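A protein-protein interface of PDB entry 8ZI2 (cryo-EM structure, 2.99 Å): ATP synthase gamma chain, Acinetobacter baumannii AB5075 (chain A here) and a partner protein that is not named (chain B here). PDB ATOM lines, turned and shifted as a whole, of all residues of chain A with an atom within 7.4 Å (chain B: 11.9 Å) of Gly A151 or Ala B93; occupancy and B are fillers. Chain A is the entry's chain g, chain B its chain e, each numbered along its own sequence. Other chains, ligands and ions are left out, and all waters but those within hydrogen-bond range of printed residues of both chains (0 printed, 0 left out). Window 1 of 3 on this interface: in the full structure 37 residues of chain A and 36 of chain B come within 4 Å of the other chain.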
ATOM      1  N   GLY A 135     -26.385 -33.243  28.182  1.00  0.00           N
ATOM      2  CA  GLY A 135     -27.177 -32.324  27.388  1.00  0.00           C
ATOM      3  C   GLY A 135     -26.688 -32.311  25.959  1.00  0.00           C
ATOM      4  O   GLY A 135     -25.548 -32.689  25.668  1.00  0.00           O
ATOM      5  N   ALA A 136     -27.570 -31.869  25.064  1.00  0.00           N
ATOM      6  CA  ALA A 136     -27.249 -31.875  23.643  1.00  0.00           C
ATOM      7  C   ALA A 136     -28.124 -30.867  22.915  1.00  0.00           C
ATOM      8  O   ALA A 136     -29.125 -30.381  23.448  1.00  0.00           O
ATOM      9  CB  ALA A 136     -27.423 -33.271  23.037  1.00  0.00           C
ATOM     10  N   THR A 137     -27.726 -30.565  21.681  1.00  0.00           N
ATOM     11  CA  THR A 137     -28.463 -29.651  20.818  1.00  0.00           C
ATOM     12  C   THR A 137     -28.101 -29.958  19.373  1.00  0.00           C
ATOM     13  O   THR A 137     -27.111 -30.640  19.094  1.00  0.00           O
ATOM     14  CB  THR A 137     -28.158 -28.186  21.144  1.00  0.00           C
ATOM     15  OG1 THR A 137     -28.804 -27.339  20.185  1.00  0.00           O
ATOM     16  CG2 THR A 137     -26.660 -27.932  21.106  1.00  0.00           C
ATOM     17  N   LEU A 146     -24.086 -17.289  20.358  1.00  0.00           N
ATOM     18  CA  LEU A 146     -23.357 -17.872  21.479  1.00  0.00           C
ATOM     19  C   LEU A 146     -24.308 -18.429  22.528  1.00  0.00           C
ATOM     20  O   LEU A 146     -24.070 -19.505  23.084  1.00  0.00           O
ATOM     21  CB  LEU A 146     -22.428 -16.830  22.102  1.00  0.00           C
ATOM     22  CG  LEU A 146     -20.998 -16.784  21.567  1.00  0.00           C
ATOM     23  CD1 LEU A 146     -20.303 -18.102  21.852  1.00  0.00           C
ATOM     24  CD2 LEU A 146     -20.964 -16.462  20.081  1.00  0.00           C
ATOM     25  N   GLU A 147     -25.400 -17.712  22.801  1.00  0.00           N
ATOM     26  CA  GLU A 147     -26.344 -18.134  23.826  1.00  0.00           C
ATOM     27  C   GLU A 147     -27.027 -19.447  23.475  1.00  0.00           C
ATOM     28  O   GLU A 147     -27.612 -20.084  24.359  1.00  0.00           O
ATOM     29  CB  GLU A 147     -27.394 -17.043  24.052  1.00  0.00           C
ATOM     30  CG  GLU A 147     -28.384 -17.367  25.159  1.00  0.00           C
ATOM     31  CD  GLU A 147     -29.380 -16.247  25.391  1.00  0.00           C
ATOM     32  OE1 GLU A 147     -29.316 -15.238  24.659  1.00  0.00           O
ATOM     33  OE2 GLU A 147     -30.199 -16.360  26.323  1.00  0.00           O
ATOM     34  N   GLN A 148     -26.973 -19.863  22.209  1.00  0.00           N
ATOM     35  CA  GLN A 148     -27.585 -21.129  21.821  1.00  0.00           C
ATOM     36  C   GLN A 148     -26.914 -22.304  22.518  1.00  0.00           C
ATOM     37  O   GLN A 148     -27.589 -23.231  22.979  1.00  0.00           O
ATOM     38  CB  GLN A 148     -27.514 -21.307  20.305  1.00  0.00           C
ATOM     39  CG  GLN A 148     -28.227 -22.535  19.777  1.00  0.00           C
ATOM     40  CD  GLN A 148     -29.722 -22.480  20.023  1.00  0.00           C
ATOM     41  OE1 GLN A 148     -30.405 -21.571  19.552  1.00  0.00           O
ATOM     42  NE2 GLN A 148     -30.236 -23.448  20.769  1.00  0.00           N
ATOM     43  N   LEU A 149     -25.585 -22.283  22.610  1.00  0.00           N
ATOM     44  CA  LEU A 149     -24.825 -23.434  23.074  1.00  0.00           C
ATOM     45  C   LEU A 149     -24.141 -23.204  24.416  1.00  0.00           C
ATOM     46  O   LEU A 149     -23.234 -23.965  24.769  1.00  0.00           O
ATOM     47  CB  LEU A 149     -23.793 -23.851  22.022  1.00  0.00           C
ATOM     48  CG  LEU A 149     -22.583 -22.969  21.696  1.00  0.00           C
ATOM     49  CD1 LEU A 149     -21.641 -23.733  20.791  1.00  0.00           C
ATOM     50  CD2 LEU A 149     -22.978 -21.666  21.026  1.00  0.00           C
ATOM     51  N   THR A 150     -24.545 -22.184  25.177  1.00  0.00           N
ATOM     52  CA  THR A 150     -24.023 -22.051  26.533  1.00  0.00           C
ATOM     53  C   THR A 150     -24.532 -23.148  27.455  1.00  0.00           C
ATOM     54  O   THR A 150     -23.943 -23.366  28.518  1.00  0.00           O
ATOM     55  CB  THR A 150     -24.381 -20.690  27.135  1.00  0.00           C
ATOM     56  OG1 THR A 150     -23.682 -20.509  28.373  1.00  0.00           O
ATOM     57  CG2 THR A 150     -25.871 -20.568  27.360  1.00  0.00           C
ATOM     58  N   GLY A 151     -25.609 -23.837  27.075  1.00  0.00           N
ATOM     59  CA  GLY A 151     -26.192 -24.826  27.966  1.00  0.00           C
ATOM     60  C   GLY A 151     -25.264 -25.992  28.245  1.00  0.00           C
ATOM     61  O   GLY A 151     -25.104 -26.410  29.394  1.00  0.00           O
ATOM     62  N   SER A 152     -24.634 -26.530  27.199  1.00  0.00           N
ATOM     63  CA  SER A 152     -23.794 -27.712  27.367  1.00  0.00           C
ATOM     64  C   SER A 152     -22.535 -27.390  28.166  1.00  0.00           C
ATOM     65  O   SER A 152     -22.175 -28.115  29.104  1.00  0.00           O
ATOM     66  CB  SER A 152     -23.436 -28.291  25.998  1.00  0.00           C
ATOM     67  OG  SER A 152     -22.747 -27.340  25.206  1.00  0.00           O
ATOM     68  N   VAL A 153     -21.850 -26.305  27.806  1.00  0.00           N
ATOM     69  CA  VAL A 153     -20.633 -25.936  28.522  1.00  0.00           C
ATOM     70  C   VAL A 153     -20.952 -25.617  29.975  1.00  0.00           C
ATOM     71  O   VAL A 153     -20.233 -26.037  30.890  1.00  0.00           O
ATOM     72  CB  VAL A 153     -19.927 -24.764  27.816  1.00  0.00           C
ATOM     73  CG1 VAL A 153     -20.921 -23.676  27.454  1.00  0.00           C
ATOM     74  CG2 VAL A 153     -18.816 -24.207  28.693  1.00  0.00           C
ATOM     75  N   GLN A 154     -22.047 -24.893  30.213  1.00  0.00           N
ATOM     76  CA  GLN A 154     -22.412 -24.546  31.582  1.00  0.00           C
ATOM     77  C   GLN A 154     -22.797 -25.781  32.388  1.00  0.00           C
ATOM     78  O   GLN A 154     -22.435 -25.891  33.563  1.00  0.00           O
ATOM     79  CB  GLN A 154     -23.546 -23.524  31.586  1.00  0.00           C
ATOM     80  CG  GLN A 154     -23.538 -22.610  32.800  1.00  0.00           C
ATOM     81  CD  GLN A 154     -24.151 -21.257  32.514  1.00  0.00           C
ATOM     82  OE1 GLN A 154     -24.689 -21.023  31.432  1.00  0.00           O
ATOM     83  NE2 GLN A 154     -24.070 -20.353  33.483  1.00  0.00           N
ATOM     84  N   VAL A 155     -23.529 -26.720  31.782  1.00  0.00           N
ATOM     85  CA  VAL A 155     -23.955 -27.896  32.532  1.00  0.00           C
ATOM     86  C   VAL A 155     -22.761 -28.784  32.859  1.00  0.00           C
ATOM     87  O   VAL A 155     -22.689 -29.366  33.948  1.00  0.00           O
ATOM     88  CB  VAL A 155     -25.064 -28.664  31.784  1.00  0.00           C
ATOM     89  CG1 VAL A 155     -24.534 -29.372  30.556  1.00  0.00           C
ATOM     90  CG2 VAL A 155     -25.735 -29.661  32.716  1.00  0.00           C
ATOM     91  N   MET A 156     -21.787 -28.886  31.950  1.00  0.00           N
ATOM     92  CA  MET A 156     -20.604 -29.679  32.276  1.00  0.00           C
ATOM     93  C   MET A 156     -19.711 -28.967  33.286  1.00  0.00           C
ATOM     94  O   MET A 156     -19.089 -29.616  34.135  1.00  0.00           O
ATOM     95  CB  MET A 156     -19.833 -30.040  31.010  1.00  0.00           C
ATOM     96  CG  MET A 156     -20.623 -30.952  30.099  1.00  0.00           C
ATOM     97  SD  MET A 156     -19.670 -32.405  29.634  1.00  0.00           S
ATOM     98  CE  MET A 156     -20.659 -33.006  28.278  1.00  0.00           C
ATOM     99  N   LEU A 157     -19.645 -27.635  33.226  1.00  0.00           N
ATOM    100  CA  LEU A 157     -18.920 -26.899  34.254  1.00  0.00           C
ATOM    101  C   LEU A 157     -19.569 -27.084  35.619  1.00  0.00           C
ATOM    102  O   LEU A 157     -18.870 -27.214  36.631  1.00  0.00           O
ATOM    103  CB  LEU A 157     -18.854 -25.419  33.882  1.00  0.00           C
ATOM    104  CG  LEU A 157     -17.855 -24.558  34.650  1.00  0.00           C
ATOM    105  CD1 LEU A 157     -16.441 -24.842  34.166  1.00  0.00           C
ATOM    106  CD2 LEU A 157     -18.194 -23.089  34.494  1.00  0.00           C
ATOM    107  N   ALA B  86     -25.450 -11.857  31.897  1.00  0.00           N
ATOM    108  CA  ALA B  86     -26.065 -12.528  33.032  1.00  0.00           C
ATOM    109  C   ALA B  86     -24.983 -13.143  33.906  1.00  0.00           C
ATOM    110  O   ALA B  86     -23.936 -13.575  33.416  1.00  0.00           O
ATOM    111  CB  ALA B  86     -27.050 -13.611  32.581  1.00  0.00           C
ATOM    112  N   ASP B  87     -25.247 -13.177  35.209  1.00  0.00           N
ATOM    113  CA  ASP B  87     -24.336 -13.757  36.189  1.00  0.00           C
ATOM    114  C   ASP B  87     -24.888 -15.114  36.603  1.00  0.00           C
ATOM    115  O   ASP B  87     -25.964 -15.193  37.206  1.00  0.00           O
ATOM    116  CB  ASP B  87     -24.171 -12.837  37.396  1.00  0.00           C
ATOM    117  CG  ASP B  87     -23.621 -11.479  37.019  1.00  0.00           C
ATOM    118  OD1 ASP B  87     -24.268 -10.779  36.212  1.00  0.00           O
ATOM    119  OD2 ASP B  87     -22.540 -11.113  37.527  1.00  0.00           O
ATOM    120  N   ASN B  88     -24.148 -16.176  36.277  1.00  0.00           N
ATOM    121  CA  ASN B  88     -24.534 -17.550  36.590  1.00  0.00           C
ATOM    122  C   ASN B  88     -25.905 -17.873  35.988  1.00  0.00           C
ATOM    123  O   ASN B  88     -26.895 -18.109  36.683  1.00  0.00           O
ATOM    124  CB  ASN B  88     -24.509 -17.791  38.104  1.00  0.00           C
ATOM    125  CG  ASN B  88     -23.102 -17.783  38.668  1.00  0.00           C
ATOM    126  OD1 ASN B  88     -22.174 -18.310  38.057  1.00  0.00           O
ATOM    127  ND2 ASN B  88     -22.939 -17.182  39.842  1.00  0.00           N
ATOM    128  N   LEU B  89     -25.927 -17.876  34.654  1.00  0.00           N
ATOM    129  CA  LEU B  89     -27.152 -18.083  33.890  1.00  0.00           C
ATOM    130  C   LEU B  89     -27.422 -19.582  33.784  1.00  0.00           C
ATOM    131  O   LEU B  89     -28.139 -20.043  32.890  1.00  0.00           O
ATOM    132  CB  LEU B  89     -27.024 -17.433  32.506  1.00  0.00           C
ATOM    133  CG  LEU B  89     -28.213 -17.389  31.541  1.00  0.00           C
ATOM    134  CD1 LEU B  89     -29.511 -17.181  32.310  1.00  0.00           C
ATOM    135  CD2 LEU B  89     -28.032 -16.330  30.465  1.00  0.00           C
ATOM    136  N   ASP B  90     -26.845 -20.350  34.712  1.00  0.00           N
ATOM    137  CA  ASP B  90     -26.937 -21.804  34.654  1.00  0.00           C
ATOM    138  C   ASP B  90     -28.380 -22.290  34.702  1.00  0.00           C
ATOM    139  O   ASP B  90     -28.691 -23.347  34.142  1.00  0.00           O
ATOM    140  CB  ASP B  90     -26.131 -22.419  35.799  1.00  0.00           C
ATOM    141  CG  ASP B  90     -25.674 -23.830  35.495  1.00  0.00           C
ATOM    142  OD1 ASP B  90     -25.849 -24.272  34.343  1.00  0.00           O
ATOM    143  OD2 ASP B  90     -25.140 -24.493  36.409  1.00  0.00           O
ATOM    144  N   GLU B  91     -29.273 -21.547  35.363  1.00  0.00           N
ATOM    145  CA  GLU B  91     -30.659 -21.995  35.464  1.00  0.00           C
ATOM    146  C   GLU B  91     -31.307 -22.102  34.089  1.00  0.00           C
ATOM    147  O   GLU B  91     -31.980 -23.096  33.790  1.00  0.00           O
ATOM    148  CB  GLU B  91     -31.462 -21.068  36.384  1.00  0.00           C
ATOM    149  CG  GLU B  91     -31.661 -19.641  35.890  1.00  0.00           C
ATOM    150  CD  GLU B  91     -30.564 -18.704  36.351  1.00  0.00           C
ATOM    151  OE1 GLU B  91     -29.524 -19.195  36.836  1.00  0.00           O
ATOM    152  OE2 GLU B  91     -30.745 -17.474  36.233  1.00  0.00           O
ATOM    153  N   ALA B  92     -31.095 -21.107  33.225  1.00  0.00           N
ATOM    154  CA  ALA B  92     -31.599 -21.213  31.861  1.00  0.00           C
ATOM    155  C   ALA B  92     -30.829 -22.260  31.071  1.00  0.00           C
ATOM    156  O   ALA B  92     -31.393 -22.893  30.174  1.00  0.00           O
ATOM    157  CB  ALA B  92     -31.534 -19.859  31.159  1.00  0.00           C
ATOM    158  N   ALA B  93     -29.550 -22.460  31.393  1.00  0.00           N
ATOM    159  CA  ALA B  93     -28.775 -23.503  30.731  1.00  0.00           C
ATOM    160  C   ALA B  93     -29.364 -24.880  31.012  1.00  0.00           C
ATOM    161  O   ALA B  93     -29.573 -25.678  30.091  1.00  0.00           O
ATOM    162  CB  ALA B  93     -27.315 -23.436  31.181  1.00  0.00           C
ATOM    163  N   ILE B  94     -29.648 -25.172  32.284  1.00  0.00           N
ATOM    164  CA  ILE B  94     -30.275 -26.448  32.621  1.00  0.00           C
ATOM    165  C   ILE B  94     -31.694 -26.515  32.074  1.00  0.00           C
ATOM    166  O   ILE B  94     -32.151 -27.587  31.661  1.00  0.00           O
ATOM    167  CB  ILE B  94     -30.246 -26.708  34.142  1.00  0.00           C
ATOM    168  CG1 ILE B  94     -28.886 -26.368  34.768  1.00  0.00           C
ATOM    169  CG2 ILE B  94     -30.597 -28.157  34.443  1.00  0.00           C
ATOM    170  CD1 ILE B  94     -27.674 -26.749  33.928  1.00  0.00           C
ATOM    171  N   LEU B  95     -32.414 -25.391  32.058  1.00  0.00           N
ATOM    172  CA  LEU B  95     -33.751 -25.391  31.473  1.00  0.00           C
ATOM    173  C   LEU B  95     -33.702 -25.813  30.010  1.00  0.00           C
ATOM    174  O   LEU B  95     -34.474 -26.673  29.574  1.00  0.00           O
ATOM    175  CB  LEU B  95     -34.392 -24.009  31.613  1.00  0.00           C
ATOM    176  CG  LEU B  95     -35.032 -23.652  32.957  1.00  0.00           C
ATOM    177  CD1 LEU B  95     -35.982 -22.477  32.796  1.00  0.00           C
ATOM    178  CD2 LEU B  95     -35.756 -24.846  33.557  1.00  0.00           C
ATOM    179  N   GLU B  96     -32.783 -25.225  29.242  1.00  0.00           N
ATOM    180  CA  GLU B  96     -32.634 -25.592  27.839  1.00  0.00           C
ATOM    181  C   GLU B  96     -32.182 -27.039  27.690  1.00  0.00           C
ATOM    182  O   GLU B  96     -32.727 -27.783  26.867  1.00  0.00           O
ATOM    183  CB  GLU B  96     -31.644 -24.643  27.162  1.00  0.00           C
ATOM    184  CG  GLU B  96     -31.671 -24.668  25.643  1.00  0.00           C
ATOM    185  CD  GLU B  96     -30.782 -25.749  25.053  1.00  0.00           C
ATOM    186  OE1 GLU B  96     -29.795 -26.138  25.713  1.00  0.00           O
ATOM    187  OE2 GLU B  96     -31.065 -26.197  23.924  1.00  0.00           O
ATOM    188  N   ALA B  97     -31.201 -27.460  28.493  1.00  0.00           N
ATOM    189  CA  ALA B  97     -30.636 -28.799  28.348  1.00  0.00           C
ATOM    190  C   ALA B  97     -31.665 -29.880  28.655  1.00  0.00           C
ATOM    191  O   ALA B  97     -31.729 -30.897  27.955  1.00  0.00           O
ATOM    192  CB  ALA B  97     -29.415 -28.950  29.254  1.00  0.00           C
ATOM    193  N   ARG B  98     -32.476 -29.680  29.692  1.00  0.00           N
ATOM    194  CA  ARG B  98     -33.441 -30.693  30.098  1.00  0.00           C
ATOM    195  C   ARG B  98     -34.674 -30.739  29.207  1.00  0.00           C
ATOM    196  O   ARG B  98     -35.432 -31.711  29.285  1.00  0.00           O
ATOM    197  CB  ARG B  98     -33.871 -30.463  31.550  1.00  0.00           C
ATOM    198  CG  ARG B  98     -32.772 -30.684  32.577  1.00  0.00           C
ATOM    199  CD  ARG B  98     -33.275 -30.486  34.000  1.00  0.00           C
ATOM    200  NE  ARG B  98     -32.208 -30.628  34.984  1.00  0.00           N
ATOM    201  CZ  ARG B  98     -32.351 -30.394  36.281  1.00  0.00           C
ATOM    202  NH1 ARG B  98     -33.507 -29.998  36.790  1.00  0.00           N
ATOM    203  NH2 ARG B  98     -31.308 -30.559  37.089  1.00  0.00           N
ATOM    204  N   LYS B  99     -34.900 -29.728  28.369  1.00  0.00           N
ATOM    205  CA  LYS B  99     -36.070 -29.718  27.501  1.00  0.00           C
ATOM    206  C   LYS B  99     -35.750 -30.039  26.046  1.00  0.00           C
ATOM    207  O   LYS B  99     -36.560 -30.682  25.374  1.00  0.00           O
ATOM    208  CB  LYS B  99     -36.794 -28.367  27.583  1.00  0.00           C
ATOM    209  CG  LYS B  99     -36.051 -27.190  26.971  1.00  0.00           C
ATOM    210  CD  LYS B  99     -36.953 -25.970  26.854  1.00  0.00           C
ATOM    211  CE  LYS B  99     -37.653 -25.662  28.168  1.00  0.00           C
ATOM    212  NZ  LYS B  99     -36.697 -25.486  29.295  1.00  0.00           N
ATOM    213  N   ASN B 100     -34.590 -29.620  25.533  1.00  0.00           N
ATOM    214  CA  ASN B 100     -34.312 -29.840  24.116  1.00  0.00           C
ATOM    215  C   ASN B 100     -33.726 -31.228  23.893  1.00  0.00           C
ATOM    216  O   ASN B 100     -34.158 -31.956  22.992  1.00  0.00           O
ATOM    217  CB  ASN B 100     -33.375 -28.755  23.572  1.00  0.00           C
ATOM    218  CG  ASN B 100     -31.910 -29.018  23.884  1.00  0.00           C
ATOM    219  OD1 ASN B 100     -31.536 -29.270  25.028  1.00  0.00           O
ATOM    220  ND2 ASN B 100     -31.072 -28.946  22.858  1.00  0.00           N
ATOM    221  N   ALA B 101     -32.749 -31.616  24.716  1.00  0.00           N
ATOM    222  CA  ALA B 101     -32.116 -32.918  24.558  1.00  0.00           C
ATOM    223  C   ALA B 101     -33.120 -34.039  24.778  1.00  0.00           C
ATOM    224  O   ALA B 101     -33.230 -34.960  23.962  1.00  0.00           O
ATOM    225  CB  ALA B 101     -30.942 -33.047  25.529  1.00  0.00           C
ATOM    226  N   GLU B 102     -33.882 -33.958  25.869  1.00  0.00           N
ATOM    227  CA  GLU B 102     -34.843 -35.008  26.185  1.00  0.00           C
ATOM    228  C   GLU B 102     -35.891 -35.146  25.088  1.00  0.00           C
ATOM    229  O   GLU B 102     -36.217 -36.263  24.671  1.00  0.00           O
ATOM    230  CB  GLU B 102     -35.498 -34.717  27.536  1.00  0.00           C
ATOM    231  CG  GLU B 102     -34.644 -35.110  28.741  1.00  0.00           C
ATOM    232  CD  GLU B 102     -33.433 -34.215  28.944  1.00  0.00           C
ATOM    233  OE1 GLU B 102     -33.247 -33.258  28.164  1.00  0.00           O
ATOM    234  OE2 GLU B 102     -32.659 -34.475  29.890  1.00  0.00           O
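Among the printed residues, merely in contact across the chains: Ala A136 with Ala B101 (3.6 Å), Thr A137 with Asn B100 (3.4 Å), Gly A151 with Ala B93 (3.7 Å), Gln A154 with Asn B88 (3.97 Å), Gln A154 with Ala B93 (3.6 Å) and Val A155 with Ile B94 (3.7 Å).
The backbone carbonyl oxygen (O) of Glu B96 lies close to the side-chain amide oxygen (OD1) of Asn B100 (2.6 Å). O of Ala B97 lies close to OD1 of Asn B100, at 3.4 Å. The side-chain hydroxyl of Thr A150 is in hydrogen-bond range of the side-chain amide oxygen of Gln A154.
The backbone NH of Leu B89 sits close to the side-chain amide nitrogen of Gln A154, 3.3 Å away. N of Asp B90 lies close to NE2 of Gln A154, 3.0 Å away. The side-chain amide nitrogen (ND2) of Asn B100 is in hydrogen-bond range of the backbone carbonyl oxygen (O) of Ala A136, 2.5 Å away.
Printed residues of chain B that touch a printed residue of chain A: Asn B88, Leu B89, Asp B90, Ala B93, Ile B94, Asn B100 and Ala B101. Hydrophobic or aromatic side chains of chain B that line the printed part of chain A: Ala B93, Ile B94 and Ala B101. Of the 15 printed residues of chain A, 5 touch a printed residue of chain B. Printed residues of chain A that touch a printed residue of chain B: Ala A136, Thr A137, Gly A151, Gln A154 and Val A155. Among the printed residues, 9 pairs touch across the chains.
No residue of chain B comes within 4 Å of Gly A135. Of the printed residues of chain B, Ala A136 touches Asn B100 and Ala B101. No residue of chain B comes within 4 Å of Leu A149. Thr A150 touches none of the printed residues of chain B. Gly A151 touches just one residue of chain B: Ala B93. No residue of chain B comes within 4 Å of Val A153. Of chain B, only Asn B88, Leu B89, Asp B90 and Ala B93 come within 4 Å of Gln A154. Of the printed residues of chain A, Asn B88 touches Gln A154. No residue of chain A comes within 4 Å of Ala B92. Ala B93 touches just these residues of chain A: Gly A151 (3.7 Å) and Gln A154 (3.6 Å). Printed residues of chain A within 4 Å of Ile B94: Val A155. Leu B95 touches none of the printed residues of chain A. Glu B96 touches none of the printed residues of chain A. Printed residues of chain A within 4 Å of Ala B101: Ala A136 (3.6 Å). The nearest residue of chain A that does not touch Ala B93 is Thr A150 (4.3 Å). The nearest printed residue of chain A that does not touch Asn B88 is Leu A157 (7.2 Å).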
